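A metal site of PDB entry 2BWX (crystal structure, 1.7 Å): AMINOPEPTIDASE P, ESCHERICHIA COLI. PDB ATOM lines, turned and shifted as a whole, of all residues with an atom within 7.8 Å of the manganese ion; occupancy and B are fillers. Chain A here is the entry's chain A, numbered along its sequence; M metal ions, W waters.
The backbone NH (N) of Glu 406 is in hydrogen-bond range of the backbone carbonyl oxygen (O) of Thr 273, 3.0 Å away.
The side-chain carboxylate (OD2) of Asp 260 sits close to the side-chain hydroxyl (OG1) of Thr 273 (3.1 Å).
OG1 of Thr 273 lies within hydrogen-bond range of NE of Arg 404 (3.3 Å).
NH2 of Arg 404 lies close to OD2 of Asp 260 (2.8 Å).
The side-chain carboxylate of Asp 260 sits close to the side-chain hydroxyl of Tyr 229.
The side-chain carboxylate (OD2) of Asp 408 sits at hydrogen-bond distance from the backbone NH (N) of Asp 271 (2.9 Å).
O of Asp 260 is in hydrogen-bond range of N of Ile 232 (2.9 Å).
The backbone NH (N) of Gly 262 lies within hydrogen-bond range of the side-chain hydroxyl (OH) of Tyr 229.
OH of Tyr 229 touches the manganese ion (3.9 Å).
OG1 of Thr 273 touches the manganese ion, 3.7 Å away.
Five residues have an atom within 4 Å of the manganese ion: Tyr 229, Asp 260, Asp 271, Thr 273 and Glu 406.
The nearest printed residue that does not touch the manganese ion is Glu 383 (4.2 Å).
The manganese ion is bound by water W3 (2.1 Å), OD1 of Asp 271 (2.2 Å), OE1 of Glu 406 (2.2 Å), OD1 of Asp 260 (2.4 Å) and OD2 of Asp 260 (2.6 Å).
The manganese ion has five donor atoms within binding distance.
Slightly farther from the manganese ion lies water W1 (2.8 Å).
Slightly farther from the manganese ion lies water W2 (2.9 Å).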
ATOM      1  N   TYR A 229      30.382  15.008 -18.163  1.00  0.00           N
ATOM      2  CA  TYR A 229      30.965  16.056 -18.995  1.00  0.00           C
ATOM      3  C   TYR A 229      31.892  16.872 -18.102  1.00  0.00           C
ATOM      4  O   TYR A 229      31.841  16.730 -16.883  1.00  0.00           O
ATOM      5  CB  TYR A 229      29.891  16.978 -19.598  1.00  0.00           C
ATOM      6  CG  TYR A 229      28.937  17.540 -18.575  1.00  0.00           C
ATOM      7  CD1 TYR A 229      27.792  16.833 -18.207  1.00  0.00           C
ATOM      8  CD2 TYR A 229      29.185  18.775 -17.954  1.00  0.00           C
ATOM      9  CE1 TYR A 229      26.920  17.330 -17.263  1.00  0.00           C
ATOM     10  CE2 TYR A 229      28.294  19.296 -17.001  1.00  0.00           C
ATOM     11  CZ  TYR A 229      27.158  18.569 -16.662  1.00  0.00           C
ATOM     12  OH  TYR A 229      26.273  19.042 -15.727  1.00  0.00           O
ATOM     13  N   ILE A 232      31.921  22.584 -14.924  1.00  0.00           N
ATOM     14  CA  ILE A 232      31.995  24.040 -15.106  1.00  0.00           C
ATOM     15  C   ILE A 232      31.809  24.693 -13.737  1.00  0.00           C
ATOM     16  O   ILE A 232      30.811  24.458 -13.055  1.00  0.00           O
ATOM     17  CB  ILE A 232      30.858  24.497 -16.053  1.00  0.00           C
ATOM     18  CG1 ILE A 232      31.083  23.940 -17.461  1.00  0.00           C
ATOM     19  CG2 ILE A 232      30.682  26.026 -16.065  1.00  0.00           C
ATOM     20  CD1 ILE A 232      29.807  23.828 -18.310  1.00  0.00           C
ATOM     21  N   LEU A 242      29.692  30.105 -21.295  1.00  0.00           N
ATOM     22  CA  LEU A 242      28.768  28.966 -21.156  1.00  0.00           C
ATOM     23  C   LEU A 242      29.424  27.623 -20.749  1.00  0.00           C
ATOM     24  O   LEU A 242      28.909  26.920 -19.874  1.00  0.00           O
ATOM     25  CB  LEU A 242      27.932  28.800 -22.437  1.00  0.00           C
ATOM     26  CG  LEU A 242      26.966  29.954 -22.751  1.00  0.00           C
ATOM     27  CD1 LEU A 242      26.156  29.660 -23.994  1.00  0.00           C
ATOM     28  CD2 LEU A 242      26.033  30.227 -21.569  1.00  0.00           C
ATOM     29  N   HIS A 243      30.519  27.268 -21.418  1.00  0.00           N
ATOM     30  CA  HIS A 243      31.276  26.038 -21.098  1.00  0.00           C
ATOM     31  C   HIS A 243      32.653  26.383 -20.504  1.00  0.00           C
ATOM     32  O   HIS A 243      33.674  25.840 -20.923  1.00  0.00           O
ATOM     33  CB  HIS A 243      31.453  25.171 -22.354  1.00  0.00           C
ATOM     34  CG  HIS A 243      30.173  24.684 -22.960  1.00  0.00           C
ATOM     35  ND1 HIS A 243      29.418  25.447 -23.829  1.00  0.00           N
ATOM     36  CD2 HIS A 243      29.527  23.502 -22.840  1.00  0.00           C
ATOM     37  CE1 HIS A 243      28.355  24.761 -24.212  1.00  0.00           C
ATOM     38  NE2 HIS A 243      28.397  23.574 -23.622  1.00  0.00           N
ATOM     39  N   LEU A 258      28.536  29.884 -10.737  1.00  0.00           N
ATOM     40  CA  LEU A 258      27.669  29.008 -11.536  1.00  0.00           C
ATOM     41  C   LEU A 258      28.392  27.669 -11.673  1.00  0.00           C
ATOM     42  O   LEU A 258      29.517  27.602 -12.181  1.00  0.00           O
ATOM     43  CB  LEU A 258      27.451  29.629 -12.902  1.00  0.00           C
ATOM     44  CG  LEU A 258      26.545  28.922 -13.915  1.00  0.00           C
ATOM     45  CD1 LEU A 258      26.063  29.947 -14.957  1.00  0.00           C
ATOM     46  CD2 LEU A 258      27.239  27.753 -14.586  1.00  0.00           C
ATOM     47  N   ILE A 259      27.721  26.620 -11.214  1.00  0.00           N
ATOM     48  CA  ILE A 259      28.299  25.278 -11.265  1.00  0.00           C
ATOM     49  C   ILE A 259      27.382  24.424 -12.141  1.00  0.00           C
ATOM     50  O   ILE A 259      26.196  24.239 -11.822  1.00  0.00           O
ATOM     51  CB  ILE A 259      28.439  24.667  -9.883  1.00  0.00           C
ATOM     52  CG1 ILE A 259      29.372  25.506  -9.013  1.00  0.00           C
ATOM     53  CG2 ILE A 259      28.984  23.250 -10.004  1.00  0.00           C
ATOM     54  CD1 ILE A 259      29.663  24.898  -7.675  1.00  0.00           C
ATOM     55  N   ASP A 260      27.945  23.921 -13.233  1.00  0.00           N
ATOM     56  CA  ASP A 260      27.274  22.995 -14.138  1.00  0.00           C
ATOM     57  C   ASP A 260      28.078  21.700 -14.078  1.00  0.00           C
ATOM     58  O   ASP A 260      29.259  21.650 -14.463  1.00  0.00           O
ATOM     59  CB  ASP A 260      27.219  23.576 -15.543  1.00  0.00           C
ATOM     60  CG  ASP A 260      26.244  22.822 -16.466  1.00  0.00           C
ATOM     61  OD1 ASP A 260      25.897  21.643 -16.199  1.00  0.00           O
ATOM     62  OD2 ASP A 260      25.828  23.423 -17.486  1.00  0.00           O
ATOM     63  N   ALA A 261      27.480  20.696 -13.433  1.00  0.00           N
ATOM     64  CA  ALA A 261      28.153  19.400 -13.222  1.00  0.00           C
ATOM     65  C   ALA A 261      27.164  18.245 -13.131  1.00  0.00           C
ATOM     66  O   ALA A 261      26.036  18.387 -12.616  1.00  0.00           O
ATOM     67  CB  ALA A 261      28.998  19.439 -11.957  1.00  0.00           C
ATOM     68  N   GLY A 262      27.604  17.092 -13.632  1.00  0.00           N
ATOM     69  CA  GLY A 262      26.788  15.894 -13.655  1.00  0.00           C
ATOM     70  C   GLY A 262      27.627  14.634 -13.625  1.00  0.00           C
ATOM     71  O   GLY A 262      28.739  14.587 -14.169  1.00  0.00           O
ATOM     72  N   GLY A 270      23.606  12.502 -15.050  1.00  0.00           N
ATOM     73  CA  GLY A 270      22.987  13.652 -14.440  1.00  0.00           C
ATOM     74  C   GLY A 270      23.519  14.919 -15.125  1.00  0.00           C
ATOM     75  O   GLY A 270      24.567  14.891 -15.810  1.00  0.00           O
ATOM     76  N   ASP A 271      22.800  16.028 -14.946  1.00  0.00           N
ATOM     77  CA  ASP A 271      23.169  17.288 -15.557  1.00  0.00           C
ATOM     78  C   ASP A 271      22.447  18.416 -14.805  1.00  0.00           C
ATOM     79  O   ASP A 271      21.315  18.737 -15.088  1.00  0.00           O
ATOM     80  CB  ASP A 271      22.821  17.246 -17.043  1.00  0.00           C
ATOM     81  CG  ASP A 271      23.298  18.451 -17.825  1.00  0.00           C
ATOM     82  OD1 ASP A 271      23.838  19.401 -17.251  1.00  0.00           O
ATOM     83  OD2 ASP A 271      23.108  18.390 -19.052  1.00  0.00           O
ATOM     84  N   ILE A 272      23.128  18.979 -13.823  1.00  0.00           N
ATOM     85  CA  ILE A 272      22.547  20.022 -12.955  1.00  0.00           C
ATOM     86  C   ILE A 272      23.384  21.292 -13.044  1.00  0.00           C
ATOM     87  O   ILE A 272      24.623  21.219 -13.107  1.00  0.00           O
ATOM     88  CB  ILE A 272      22.480  19.570 -11.468  1.00  0.00           C
ATOM     89  CG1 ILE A 272      21.452  18.429 -11.243  1.00  0.00           C
ATOM     90  CG2 ILE A 272      22.146  20.749 -10.552  1.00  0.00           C
ATOM     91  CD1 ILE A 272      21.406  17.951  -9.787  1.00  0.00           C
ATOM     92  N   THR A 273      22.704  22.449 -13.072  1.00  0.00           N
ATOM     93  CA  THR A 273      23.345  23.740 -12.862  1.00  0.00           C
ATOM     94  C   THR A 273      22.676  24.417 -11.671  1.00  0.00           C
ATOM     95  O   THR A 273      21.434  24.441 -11.541  1.00  0.00           O
ATOM     96  CB  THR A 273      23.303  24.666 -14.095  1.00  0.00           C
ATOM     97  OG1 THR A 273      23.767  23.965 -15.261  1.00  0.00           O
ATOM     98  CG2 THR A 273      24.179  25.910 -13.874  1.00  0.00           C
ATOM     99  N   VAL A 360      24.704  13.404 -22.116  1.00  0.00           N
ATOM    100  CA  VAL A 360      24.142  14.732 -22.071  1.00  0.00           C
ATOM    101  C   VAL A 360      24.049  15.216 -23.522  1.00  0.00           C
ATOM    102  O   VAL A 360      24.834  14.802 -24.381  1.00  0.00           O
ATOM    103  CB  VAL A 360      24.972  15.700 -21.194  1.00  0.00           C
ATOM    104  CG1 VAL A 360      24.954  15.235 -19.745  1.00  0.00           C
ATOM    105  CG2 VAL A 360      26.401  15.848 -21.721  1.00  0.00           C
ATOM    106  N   HIS A 361      23.080  16.090 -23.781  1.00  0.00           N
ATOM    107  CA  HIS A 361      22.687  16.389 -25.138  1.00  0.00           C
ATOM    108  C   HIS A 361      22.476  15.061 -25.836  1.00  0.00           C
ATOM    109  O   HIS A 361      23.149  14.712 -26.819  1.00  0.00           O
ATOM    110  CB  HIS A 361      23.743  17.232 -25.860  1.00  0.00           C
ATOM    111  CG  HIS A 361      23.924  18.582 -25.249  1.00  0.00           C
ATOM    112  ND1 HIS A 361      24.950  19.434 -25.604  1.00  0.00           N
ATOM    113  CD2 HIS A 361      23.224  19.231 -24.281  1.00  0.00           C
ATOM    114  CE1 HIS A 361      24.860  20.545 -24.908  1.00  0.00           C
ATOM    115  NE2 HIS A 361      23.814  20.458 -24.096  1.00  0.00           N
ATOM    116  N   THR A 381      16.612  18.064 -19.952  1.00  0.00           N
ATOM    117  CA  THR A 381      17.022  19.127 -19.056  1.00  0.00           C
ATOM    118  C   THR A 381      16.090  20.322 -19.206  1.00  0.00           C
ATOM    119  O   THR A 381      15.388  20.479 -20.207  1.00  0.00           O
ATOM    120  CB  THR A 381      18.458  19.622 -19.368  1.00  0.00           C
ATOM    121  OG1 THR A 381      18.446  20.264 -20.655  1.00  0.00           O
ATOM    122  CG2 THR A 381      19.445  18.462 -19.345  1.00  0.00           C
ATOM    123  N   GLU A 383      16.886  24.346 -18.497  1.00  0.00           N
ATOM    124  CA  GLU A 383      18.088  25.117 -18.180  1.00  0.00           C
ATOM    125  C   GLU A 383      18.032  26.575 -18.636  1.00  0.00           C
ATOM    126  O   GLU A 383      18.903  27.033 -19.372  1.00  0.00           O
ATOM    127  CB  GLU A 383      19.360  24.413 -18.715  1.00  0.00           C
ATOM    128  CG  GLU A 383      19.350  24.029 -20.204  1.00  0.00           C
ATOM    129  CD  GLU A 383      20.605  23.224 -20.575  1.00  0.00           C
ATOM    130  OE1 GLU A 383      21.688  23.783 -20.314  1.00  0.00           O
ATOM    131  OE2 GLU A 383      20.504  22.052 -21.077  1.00  0.00           O
ATOM    132  N   ARG A 404      22.551  30.465 -14.390  1.00  0.00           N
ATOM    133  CA  ARG A 404      21.766  29.390 -14.976  1.00  0.00           C
ATOM    134  C   ARG A 404      21.307  28.461 -13.866  1.00  0.00           C
ATOM    135  O   ARG A 404      22.009  28.271 -12.867  1.00  0.00           O
ATOM    136  CB  ARG A 404      22.602  28.643 -16.035  1.00  0.00           C
ATOM    137  CG  ARG A 404      21.966  27.368 -16.548  1.00  0.00           C
ATOM    138  CD  ARG A 404      22.619  26.841 -17.821  1.00  0.00           C
ATOM    139  NE  ARG A 404      23.945  26.266 -17.636  1.00  0.00           N
ATOM    140  CZ  ARG A 404      25.110  26.855 -17.942  1.00  0.00           C
ATOM    141  NH1 ARG A 404      25.173  28.095 -18.396  1.00  0.00           N
ATOM    142  NH2 ARG A 404      26.249  26.201 -17.752  1.00  0.00           N
ATOM    143  N   GLU A 406      19.327  24.644 -13.629  1.00  0.00           N
ATOM    144  CA  GLU A 406      19.016  23.529 -14.503  1.00  0.00           C
ATOM    145  C   GLU A 406      18.632  22.315 -13.672  1.00  0.00           C
ATOM    146  O   GLU A 406      19.370  21.899 -12.758  1.00  0.00           O
ATOM    147  CB  GLU A 406      20.225  23.219 -15.392  1.00  0.00           C
ATOM    148  CG  GLU A 406      20.152  21.902 -16.141  1.00  0.00           C
ATOM    149  CD  GLU A 406      21.364  21.676 -17.009  1.00  0.00           C
ATOM    150  OE1 GLU A 406      22.474  22.101 -16.607  1.00  0.00           O
ATOM    151  OE2 GLU A 406      21.194  21.093 -18.091  1.00  0.00           O
ATOM    152  N   ASP A 407      17.490  21.736 -14.025  1.00  0.00           N
ATOM    153  CA  ASP A 407      17.017  20.462 -13.472  1.00  0.00           C
ATOM    154  C   ASP A 407      16.861  19.451 -14.629  1.00  0.00           C
ATOM    155  O   ASP A 407      16.799  19.842 -15.806  1.00  0.00           O
ATOM    156  CB  ASP A 407      15.670  20.630 -12.752  1.00  0.00           C
ATOM    157  CG  ASP A 407      15.797  21.164 -11.314  1.00  0.00           C
ATOM    158  OD1 ASP A 407      16.877  20.958 -10.668  1.00  0.00           O
ATOM    159  OD2 ASP A 407      14.817  21.795 -10.853  1.00  0.00           O
ATOM    160  N   ASP A 408      16.805  18.179 -14.261  1.00  0.00           N
ATOM    161  CA  ASP A 408      16.560  17.072 -15.186  1.00  0.00           C
ATOM    162  C   ASP A 408      15.197  16.503 -14.850  1.00  0.00           C
ATOM    163  O   ASP A 408      14.895  16.263 -13.665  1.00  0.00           O
ATOM    164  CB  ASP A 408      17.625  15.992 -15.038  1.00  0.00           C
ATOM    165  CG  ASP A 408      19.014  16.559 -15.109  1.00  0.00           C
ATOM    166  OD1 ASP A 408      19.187  17.550 -15.871  1.00  0.00           O
ATOM    167  OD2 ASP A 408      19.919  16.019 -14.425  1.00  0.00           O
HETATM  168 MN    MN M   1      24.196  21.460 -17.903  1.00  0.00          MN
HETATM  169  O   HOH W   1      26.187  20.442 -19.558  1.00  0.00           O
HETATM  170  O   HOH W   2      22.750  20.623 -20.229  1.00  0.00           O
HETATM  171  O   HOH W   3      23.901  22.904 -19.462  1.00  0.00           O
